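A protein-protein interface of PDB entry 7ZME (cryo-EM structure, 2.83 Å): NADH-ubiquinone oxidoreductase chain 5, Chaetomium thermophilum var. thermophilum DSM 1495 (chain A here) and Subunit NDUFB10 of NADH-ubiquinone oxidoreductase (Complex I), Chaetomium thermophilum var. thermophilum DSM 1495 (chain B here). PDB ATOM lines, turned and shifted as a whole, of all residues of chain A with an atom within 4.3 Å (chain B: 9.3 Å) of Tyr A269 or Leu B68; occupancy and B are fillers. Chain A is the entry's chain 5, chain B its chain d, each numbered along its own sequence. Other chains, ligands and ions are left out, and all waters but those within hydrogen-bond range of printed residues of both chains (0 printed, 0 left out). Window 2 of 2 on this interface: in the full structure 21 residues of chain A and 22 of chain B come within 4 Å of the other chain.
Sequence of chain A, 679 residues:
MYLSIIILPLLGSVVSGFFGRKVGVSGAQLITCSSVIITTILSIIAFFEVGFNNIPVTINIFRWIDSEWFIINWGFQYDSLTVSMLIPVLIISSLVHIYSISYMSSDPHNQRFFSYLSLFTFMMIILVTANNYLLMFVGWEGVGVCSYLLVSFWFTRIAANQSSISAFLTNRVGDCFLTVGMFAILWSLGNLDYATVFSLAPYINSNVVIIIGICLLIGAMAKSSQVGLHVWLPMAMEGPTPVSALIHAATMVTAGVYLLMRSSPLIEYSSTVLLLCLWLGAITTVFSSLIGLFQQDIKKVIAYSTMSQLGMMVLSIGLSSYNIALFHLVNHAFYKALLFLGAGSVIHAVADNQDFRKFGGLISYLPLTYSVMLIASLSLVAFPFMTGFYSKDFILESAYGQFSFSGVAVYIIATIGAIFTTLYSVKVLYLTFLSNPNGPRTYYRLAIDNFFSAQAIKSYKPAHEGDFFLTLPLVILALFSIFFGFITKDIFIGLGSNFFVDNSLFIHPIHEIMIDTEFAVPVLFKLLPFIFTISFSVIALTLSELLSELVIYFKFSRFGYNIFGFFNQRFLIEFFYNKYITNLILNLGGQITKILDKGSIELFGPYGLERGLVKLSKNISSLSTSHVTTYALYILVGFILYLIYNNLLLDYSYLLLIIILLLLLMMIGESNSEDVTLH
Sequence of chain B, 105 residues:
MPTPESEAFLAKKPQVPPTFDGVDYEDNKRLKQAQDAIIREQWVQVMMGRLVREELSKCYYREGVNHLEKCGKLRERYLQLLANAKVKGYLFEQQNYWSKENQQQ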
ATOM      1  N   SER A 199      -3.683  -7.212  -9.078  1.00  0.00           N
ATOM      2  CA  SER A 199      -5.093  -6.934  -9.310  1.00  0.00           C
ATOM      3  C   SER A 199      -5.954  -8.151  -9.005  1.00  0.00           C
ATOM      4  O   SER A 199      -7.075  -8.017  -8.505  1.00  0.00           O
ATOM      5  CB  SER A 199      -5.302  -6.487 -10.749  1.00  0.00           C
ATOM      6  OG  SER A 199      -4.740  -7.438 -11.629  1.00  0.00           O
ATOM      7  N   ALA A 201      -5.005 -10.846  -7.033  1.00  0.00           N
ATOM      8  CA  ALA A 201      -4.650 -11.568  -5.812  1.00  0.00           C
ATOM      9  C   ALA A 201      -5.794 -11.746  -4.816  1.00  0.00           C
ATOM     10  O   ALA A 201      -5.902 -12.845  -4.247  1.00  0.00           O
ATOM     11  CB  ALA A 201      -3.457 -10.879  -5.137  1.00  0.00           C
ATOM     12  N   PRO A 202      -6.650 -10.755  -4.540  1.00  0.00           N
ATOM     13  CA  PRO A 202      -7.711 -10.972  -3.542  1.00  0.00           C
ATOM     14  C   PRO A 202      -8.692 -12.072  -3.898  1.00  0.00           C
ATOM     15  O   PRO A 202      -9.331 -12.623  -2.996  1.00  0.00           O
ATOM     16  CB  PRO A 202      -8.416  -9.612  -3.473  1.00  0.00           C
ATOM     17  CG  PRO A 202      -8.011  -8.899  -4.689  1.00  0.00           C
ATOM     18  CD  PRO A 202      -6.637  -9.356  -4.998  1.00  0.00           C
ATOM     19  N   TYR A 203      -8.836 -12.415  -5.172  1.00  0.00           N
ATOM     20  CA  TYR A 203      -9.828 -13.385  -5.603  1.00  0.00           C
ATOM     21  C   TYR A 203      -9.245 -14.767  -5.825  1.00  0.00           C
ATOM     22  O   TYR A 203      -9.962 -15.659  -6.282  1.00  0.00           O
ATOM     23  CB  TYR A 203     -10.499 -12.907  -6.886  1.00  0.00           C
ATOM     24  CG  TYR A 203     -10.879 -11.456  -6.851  1.00  0.00           C
ATOM     25  CD1 TYR A 203     -12.047 -11.044  -6.239  1.00  0.00           C
ATOM     26  CD2 TYR A 203     -10.067 -10.498  -7.430  1.00  0.00           C
ATOM     27  CE1 TYR A 203     -12.400  -9.720  -6.208  1.00  0.00           C
ATOM     28  CE2 TYR A 203     -10.409  -9.173  -7.403  1.00  0.00           C
ATOM     29  CZ  TYR A 203     -11.578  -8.788  -6.792  1.00  0.00           C
ATOM     30  OH  TYR A 203     -11.922  -7.461  -6.770  1.00  0.00           O
ATOM     31  N   VAL A 209      -1.933 -18.793  -2.534  1.00  0.00           N
ATOM     32  CA  VAL A 209      -1.257 -17.606  -2.026  1.00  0.00           C
ATOM     33  C   VAL A 209      -0.265 -17.991  -0.937  1.00  0.00           C
ATOM     34  O   VAL A 209       0.832 -17.429  -0.850  1.00  0.00           O
ATOM     35  CB  VAL A 209      -2.288 -16.579  -1.526  1.00  0.00           C
ATOM     36  CG1 VAL A 209      -1.592 -15.356  -0.945  1.00  0.00           C
ATOM     37  CG2 VAL A 209      -3.211 -16.174  -2.652  1.00  0.00           C
ATOM     38  N   PRO A 265       0.769  -6.530  -2.114  1.00  0.00           N
ATOM     39  CA  PRO A 265      -0.622  -6.787  -2.519  1.00  0.00           C
ATOM     40  C   PRO A 265      -0.992  -8.258  -2.531  1.00  0.00           C
ATOM     41  O   PRO A 265      -2.148  -8.593  -2.244  1.00  0.00           O
ATOM     42  CB  PRO A 265      -0.690  -6.178  -3.921  1.00  0.00           C
ATOM     43  CG  PRO A 265       0.331  -5.130  -3.912  1.00  0.00           C
ATOM     44  CD  PRO A 265       1.454  -5.690  -3.113  1.00  0.00           C
ATOM     45  N   LEU A 266      -0.055  -9.151  -2.850  1.00  0.00           N
ATOM     46  CA  LEU A 266      -0.365 -10.576  -2.841  1.00  0.00           C
ATOM     47  C   LEU A 266      -0.314 -11.163  -1.437  1.00  0.00           C
ATOM     48  O   LEU A 266      -1.192 -11.945  -1.060  1.00  0.00           O
ATOM     49  CB  LEU A 266       0.596 -11.335  -3.759  1.00  0.00           C
ATOM     50  CG  LEU A 266       0.335 -12.837  -3.904  1.00  0.00           C
ATOM     51  CD1 LEU A 266       0.493 -13.272  -5.341  1.00  0.00           C
ATOM     52  CD2 LEU A 266       1.267 -13.640  -3.011  1.00  0.00           C
ATOM     53  N   ILE A 267       0.701 -10.804  -0.650  1.00  0.00           N
ATOM     54  CA  ILE A 267       0.899 -11.467   0.634  1.00  0.00           C
ATOM     55  C   ILE A 267      -0.010 -10.911   1.718  1.00  0.00           C
ATOM     56  O   ILE A 267      -0.162 -11.543   2.769  1.00  0.00           O
ATOM     57  CB  ILE A 267       2.371 -11.373   1.066  1.00  0.00           C
ATOM     58  CG1 ILE A 267       2.743  -9.935   1.415  1.00  0.00           C
ATOM     59  CG2 ILE A 267       3.272 -11.877  -0.040  1.00  0.00           C
ATOM     60  CD1 ILE A 267       4.143  -9.787   1.961  1.00  0.00           C
ATOM     61  N   GLU A 268      -0.625  -9.748   1.493  1.00  0.00           N
ATOM     62  CA  GLU A 268      -1.616  -9.236   2.429  1.00  0.00           C
ATOM     63  C   GLU A 268      -2.826 -10.148   2.544  1.00  0.00           C
ATOM     64  O   GLU A 268      -3.514 -10.122   3.571  1.00  0.00           O
ATOM     65  CB  GLU A 268      -2.063  -7.837   2.013  1.00  0.00           C
ATOM     66  CG  GLU A 268      -1.291  -6.721   2.677  1.00  0.00           C
ATOM     67  CD  GLU A 268      -1.571  -6.640   4.161  1.00  0.00           C
ATOM     68  OE1 GLU A 268      -2.542  -5.958   4.544  1.00  0.00           O
ATOM     69  OE2 GLU A 268      -0.823  -7.255   4.948  1.00  0.00           O
ATOM     70  N   TYR A 269      -3.097 -10.960   1.520  1.00  0.00           N
ATOM     71  CA  TYR A 269      -4.232 -11.871   1.517  1.00  0.00           C
ATOM     72  C   TYR A 269      -3.869 -13.256   2.026  1.00  0.00           C
ATOM     73  O   TYR A 269      -4.494 -14.246   1.625  1.00  0.00           O
ATOM     74  CB  TYR A 269      -4.834 -11.948   0.116  1.00  0.00           C
ATOM     75  CG  TYR A 269      -5.421 -10.633  -0.330  1.00  0.00           C
ATOM     76  CD1 TYR A 269      -6.605 -10.164   0.213  1.00  0.00           C
ATOM     77  CD2 TYR A 269      -4.781  -9.850  -1.276  1.00  0.00           C
ATOM     78  CE1 TYR A 269      -7.141  -8.960  -0.178  1.00  0.00           C
ATOM     79  CE2 TYR A 269      -5.313  -8.640  -1.676  1.00  0.00           C
ATOM     80  CZ  TYR A 269      -6.492  -8.201  -1.120  1.00  0.00           C
ATOM     81  OH  TYR A 269      -7.032  -7.001  -1.513  1.00  0.00           O
ATOM     82  N   SER A 270      -2.862 -13.352   2.895  1.00  0.00           N
ATOM     83  CA  SER A 270      -2.575 -14.600   3.600  1.00  0.00           C
ATOM     84  C   SER A 270      -1.831 -14.218   4.880  1.00  0.00           C
ATOM     85  O   SER A 270      -0.654 -13.854   4.826  1.00  0.00           O
ATOM     86  CB  SER A 270      -1.762 -15.555   2.747  1.00  0.00           C
ATOM     87  OG  SER A 270      -0.379 -15.320   2.908  1.00  0.00           O
ATOM     88  N   PHE A 506       0.738  -2.024  -0.245  1.00  0.00           N
ATOM     89  CA  PHE A 506      -0.666  -2.309   0.014  1.00  0.00           C
ATOM     90  C   PHE A 506      -0.848  -2.795   1.445  1.00  0.00           C
ATOM     91  O   PHE A 506      -0.190  -3.748   1.871  1.00  0.00           O
ATOM     92  CB  PHE A 506      -1.195  -3.354  -0.969  1.00  0.00           C
ATOM     93  CG  PHE A 506      -2.581  -3.833  -0.658  1.00  0.00           C
ATOM     94  CD1 PHE A 506      -3.665  -2.988  -0.799  1.00  0.00           C
ATOM     95  CD2 PHE A 506      -2.799  -5.127  -0.226  1.00  0.00           C
ATOM     96  CE1 PHE A 506      -4.939  -3.424  -0.513  1.00  0.00           C
ATOM     97  CE2 PHE A 506      -4.070  -5.571   0.063  1.00  0.00           C
ATOM     98  CZ  PHE A 506      -5.142  -4.718  -0.080  1.00  0.00           C
ATOM     99  N   HIS A 508      -4.028  -3.838   4.176  1.00  0.00           N
ATOM    100  CA  HIS A 508      -5.482  -4.136   4.242  1.00  0.00           C
ATOM    101  C   HIS A 508      -6.101  -3.555   5.529  1.00  0.00           C
ATOM    102  O   HIS A 508      -5.477  -3.717   6.591  1.00  0.00           O
ATOM    103  CB  HIS A 508      -5.785  -5.627   4.062  1.00  0.00           C
ATOM    104  CG  HIS A 508      -7.127  -5.866   3.462  1.00  0.00           C
ATOM    105  ND1 HIS A 508      -8.265  -5.994   4.230  1.00  0.00           N
ATOM    106  CD2 HIS A 508      -7.522  -5.967   2.176  1.00  0.00           C
ATOM    107  CE1 HIS A 508      -9.303  -6.185   3.447  1.00  0.00           C
ATOM    108  NE2 HIS A 508      -8.873  -6.168   2.180  1.00  0.00           N
ATOM    109  N   CYS B  59      -5.430  -0.204 -16.555  1.00  0.00           N
ATOM    110  CA  CYS B  59      -6.360   0.225 -15.517  1.00  0.00           C
ATOM    111  C   CYS B  59      -5.690   0.238 -14.150  1.00  0.00           C
ATOM    112  O   CYS B  59      -5.914   1.152 -13.347  1.00  0.00           O
ATOM    113  CB  CYS B  59      -7.583  -0.693 -15.506  1.00  0.00           C
ATOM    114  SG  CYS B  59      -9.015  -0.079 -14.575  1.00  0.00           S
ATOM    115  N   TYR B  60      -4.863  -0.770 -13.872  1.00  0.00           N
ATOM    116  CA  TYR B  60      -4.267  -0.919 -12.548  1.00  0.00           C
ATOM    117  C   TYR B  60      -3.387   0.272 -12.191  1.00  0.00           C
ATOM    118  O   TYR B  60      -3.491   0.829 -11.093  1.00  0.00           O
ATOM    119  CB  TYR B  60      -3.465  -2.218 -12.495  1.00  0.00           C
ATOM    120  CG  TYR B  60      -2.790  -2.458 -11.174  1.00  0.00           C
ATOM    121  CD1 TYR B  60      -3.518  -2.884 -10.080  1.00  0.00           C
ATOM    122  CD2 TYR B  60      -1.428  -2.250 -11.020  1.00  0.00           C
ATOM    123  CE1 TYR B  60      -2.913  -3.101  -8.873  1.00  0.00           C
ATOM    124  CE2 TYR B  60      -0.813  -2.465  -9.812  1.00  0.00           C
ATOM    125  CZ  TYR B  60      -1.562  -2.892  -8.740  1.00  0.00           C
ATOM    126  OH  TYR B  60      -0.966  -3.117  -7.523  1.00  0.00           O
ATOM    127  N   GLU B  63      -5.599   3.590 -11.854  1.00  0.00           N
ATOM    128  CA  GLU B  63      -6.483   3.780 -10.711  1.00  0.00           C
ATOM    129  C   GLU B  63      -5.721   3.809  -9.390  1.00  0.00           C
ATOM    130  O   GLU B  63      -5.956   4.690  -8.559  1.00  0.00           O
ATOM    131  CB  GLU B  63      -7.550   2.683 -10.688  1.00  0.00           C
ATOM    132  CG  GLU B  63      -8.673   2.894 -11.693  1.00  0.00           C
ATOM    133  CD  GLU B  63      -9.104   4.345 -11.816  1.00  0.00           C
ATOM    134  OE1 GLU B  63      -9.423   4.975 -10.787  1.00  0.00           O
ATOM    135  OE2 GLU B  63      -9.118   4.862 -12.952  1.00  0.00           O
ATOM    136  N   GLY B  64      -4.818   2.859  -9.176  1.00  0.00           N
ATOM    137  CA  GLY B  64      -4.016   2.848  -7.969  1.00  0.00           C
ATOM    138  C   GLY B  64      -4.737   2.301  -6.754  1.00  0.00           C
ATOM    139  O   GLY B  64      -4.951   1.093  -6.642  1.00  0.00           O
ATOM    140  N   VAL B  65      -5.094   3.190  -5.826  1.00  0.00           N
ATOM    141  CA  VAL B  65      -5.850   2.783  -4.645  1.00  0.00           C
ATOM    142  C   VAL B  65      -7.168   2.142  -5.049  1.00  0.00           C
ATOM    143  O   VAL B  65      -7.508   1.039  -4.605  1.00  0.00           O
ATOM    144  CB  VAL B  65      -6.082   3.994  -3.725  1.00  0.00           C
ATOM    145  CG1 VAL B  65      -6.953   3.618  -2.574  1.00  0.00           C
ATOM    146  CG2 VAL B  65      -4.786   4.467  -3.187  1.00  0.00           C
ATOM    147  N   ASN B  66      -7.923   2.822  -5.902  1.00  0.00           N
ATOM    148  CA  ASN B  66      -9.238   2.355  -6.328  1.00  0.00           C
ATOM    149  C   ASN B  66      -9.180   1.527  -7.609  1.00  0.00           C
ATOM    150  O   ASN B  66      -9.923   1.757  -8.557  1.00  0.00           O
ATOM    151  CB  ASN B  66     -10.177   3.549  -6.459  1.00  0.00           C
ATOM    152  CG  ASN B  66      -9.733   4.537  -7.524  1.00  0.00           C
ATOM    153  OD1 ASN B  66      -8.782   4.294  -8.262  1.00  0.00           O
ATOM    154  ND2 ASN B  66     -10.427   5.665  -7.604  1.00  0.00           N
ATOM    155  N   HIS B  67      -8.301   0.526  -7.631  1.00  0.00           N
ATOM    156  CA  HIS B  67      -8.304  -0.460  -8.701  1.00  0.00           C
ATOM    157  C   HIS B  67      -9.183  -1.650  -8.368  1.00  0.00           C
ATOM    158  O   HIS B  67      -9.717  -2.294  -9.275  1.00  0.00           O
ATOM    159  CB  HIS B  67      -6.885  -0.966  -8.983  1.00  0.00           C
ATOM    160  CG  HIS B  67      -6.386  -1.965  -7.986  1.00  0.00           C
ATOM    161  ND1 HIS B  67      -6.535  -3.324  -8.163  1.00  0.00           N
ATOM    162  CD2 HIS B  67      -5.759  -1.809  -6.797  1.00  0.00           C
ATOM    163  CE1 HIS B  67      -6.009  -3.960  -7.135  1.00  0.00           C
ATOM    164  NE2 HIS B  67      -5.536  -3.064  -6.289  1.00  0.00           N
ATOM    165  N   LEU B  68      -9.344  -1.942  -7.076  1.00  0.00           N
ATOM    166  CA  LEU B  68     -10.160  -3.057  -6.629  1.00  0.00           C
ATOM    167  C   LEU B  68     -11.647  -2.808  -6.828  1.00  0.00           C
ATOM    168  O   LEU B  68     -12.436  -3.746  -6.693  1.00  0.00           O
ATOM    169  CB  LEU B  68      -9.864  -3.350  -5.161  1.00  0.00           C
ATOM    170  CG  LEU B  68      -8.682  -4.287  -4.925  1.00  0.00           C
ATOM    171  CD1 LEU B  68      -8.518  -4.595  -3.450  1.00  0.00           C
ATOM    172  CD2 LEU B  68      -8.862  -5.564  -5.729  1.00  0.00           C
ATOM    173  N   GLU B  69     -12.047  -1.579  -7.153  1.00  0.00           N
ATOM    174  CA  GLU B  69     -13.441  -1.280  -7.423  1.00  0.00           C
ATOM    175  C   GLU B  69     -13.675  -0.612  -8.766  1.00  0.00           C
ATOM    176  O   GLU B  69     -14.825  -0.285  -9.081  1.00  0.00           O
ATOM    177  CB  GLU B  69     -14.027  -0.398  -6.313  1.00  0.00           C
ATOM    178  CG  GLU B  69     -13.635   1.061  -6.387  1.00  0.00           C
ATOM    179  CD  GLU B  69     -14.547   1.940  -5.557  1.00  0.00           C
ATOM    180  OE1 GLU B  69     -15.698   1.528  -5.299  1.00  0.00           O
ATOM    181  OE2 GLU B  69     -14.111   3.037  -5.153  1.00  0.00           O
ATOM    182  N   LYS B  70     -12.635  -0.403  -9.569  1.00  0.00           N
ATOM    183  CA  LYS B  70     -12.798   0.240 -10.861  1.00  0.00           C
ATOM    184  C   LYS B  70     -12.231  -0.566 -12.018  1.00  0.00           C
ATOM    185  O   LYS B  70     -12.366  -0.139 -13.169  1.00  0.00           O
ATOM    186  CB  LYS B  70     -12.150   1.633 -10.847  1.00  0.00           C
ATOM    187  CG  LYS B  70     -12.919   2.649 -10.022  1.00  0.00           C
ATOM    188  CD  LYS B  70     -12.385   4.053 -10.232  1.00  0.00           C
ATOM    189  CE  LYS B  70     -12.825   4.618 -11.571  1.00  0.00           C
ATOM    190  NZ  LYS B  70     -12.234   5.961 -11.824  1.00  0.00           N
ATOM    191  N   CYS B  71     -11.607  -1.713 -11.755  1.00  0.00           N
ATOM    192  CA  CYS B  71     -10.989  -2.523 -12.796  1.00  0.00           C
ATOM    193  C   CYS B  71     -11.472  -3.965 -12.719  1.00  0.00           C
ATOM    194  O   CYS B  71     -10.778  -4.884 -13.161  1.00  0.00           O
ATOM    195  CB  CYS B  71      -9.464  -2.461 -12.703  1.00  0.00           C
ATOM    196  SG  CYS B  71      -8.755  -0.794 -12.690  1.00  0.00           S
ATOM    197  N   GLY B  72     -12.664  -4.177 -12.157  1.00  0.00           N
ATOM    198  CA  GLY B  72     -13.194  -5.521 -12.015  1.00  0.00           C
ATOM    199  C   GLY B  72     -13.829  -6.082 -13.263  1.00  0.00           C
ATOM    200  O   GLY B  72     -13.962  -7.304 -13.378  1.00  0.00           O
ATOM    201  N   LYS B  73     -14.231  -5.222 -14.198  1.00  0.00           N
ATOM    202  CA  LYS B  73     -14.815  -5.710 -15.442  1.00  0.00           C
ATOM    203  C   LYS B  73     -13.815  -6.553 -16.219  1.00  0.00           C
ATOM    204  O   LYS B  73     -14.169  -7.600 -16.771  1.00  0.00           O
ATOM    205  CB  LYS B  73     -15.302  -4.535 -16.290  1.00  0.00           C
ATOM    206  CG  LYS B  73     -15.999  -4.946 -17.575  1.00  0.00           C
ATOM    207  CD  LYS B  73     -17.284  -5.699 -17.282  1.00  0.00           C
ATOM    208  CE  LYS B  73     -18.290  -4.811 -16.570  1.00  0.00           C
ATOM    209  NZ  LYS B  73     -18.800  -3.730 -17.456  1.00  0.00           N
ATOM    210  N   ARG B  75     -11.214  -7.988 -14.756  1.00  0.00           N
ATOM    211  CA  ARG B  75     -10.767  -9.075 -13.891  1.00  0.00           C
ATOM    212  C   ARG B  75     -11.565 -10.349 -14.131  1.00  0.00           C
ATOM    213  O   ARG B  75     -10.990 -11.441 -14.173  1.00  0.00           O
ATOM    214  CB  ARG B  75     -10.839  -8.648 -12.429  1.00  0.00           C
ATOM    215  CG  ARG B  75      -9.639  -7.835 -11.993  1.00  0.00           C
ATOM    216  CD  ARG B  75      -9.599  -7.663 -10.495  1.00  0.00           C
ATOM    217  NE  ARG B  75      -9.976  -6.312 -10.106  1.00  0.00           N
ATOM    218  CZ  ARG B  75     -11.101  -6.007  -9.475  1.00  0.00           C
ATOM    219  NH1 ARG B  75     -11.366  -4.749  -9.168  1.00  0.00           N
ATOM    220  NH2 ARG B  75     -11.972  -6.953  -9.173  1.00  0.00           N
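Of the printed residues of chain B, Tyr A269 touches Leu B68 (3.4 Å). Of chain B, only Leu B68 comes within 4 Å of Pro A202. No residue of chain B comes within 4 Å of Ser A270. Printed residues of chain A within 4 Å of Arg B75: Ser A199 and Tyr A203. Printed residues of chain B within 4 Å of Tyr A203: Leu B68 and Arg B75. Printed residues of chain A within 4 Å of His B67: Ser A199. Of the printed residues of chain B, Ser A199 touches His B67 (3.8 Å) and Arg B75 (3.2 Å). Lys B73 touches none of the printed residues of chain A. Val A209 touches none of the printed residues of chain B. The nearest residue of chain A that does not touch Leu B68 is Ser A199 (4.1 Å).
The guanidinium group (NH2) of Arg B75 lies within hydrogen-bond range of the side-chain hydroxyl (OH) of Tyr A203, 2.5 Å away.
Of the 14 printed residues of chain B, 3 touch a printed residue of chain A. Hydrophobic or aromatic side chains of chain A that line the printed part of chain B: Pro A202, Tyr A203 and Tyr A269.
Ser A199 touches His B67. O of Ser A199 touches CD of Arg B75 (3.2 Å). Pro A202 touches Leu B68 (CG to CD2, 3.6 Å). CD2 of Leu B68 touches OH of Tyr A203, 3.7 Å away. OH of Tyr A269 touches CD1 of Leu B68, at 3.4 Å.
NH1 of Arg B75 sits at hydrogen-bond distance from O of His B67 (3.0 Å). The side-chain sulfur of Cys B59 is disulfide-bonded to the side-chain sulfur of Cys B71 (2.0 Å). O of Cys B71 sits close to NE of Arg B75, 3.5 Å away. O of Leu B68 sits at hydrogen-bond distance from NH1 of Arg B75 (2.9 Å).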
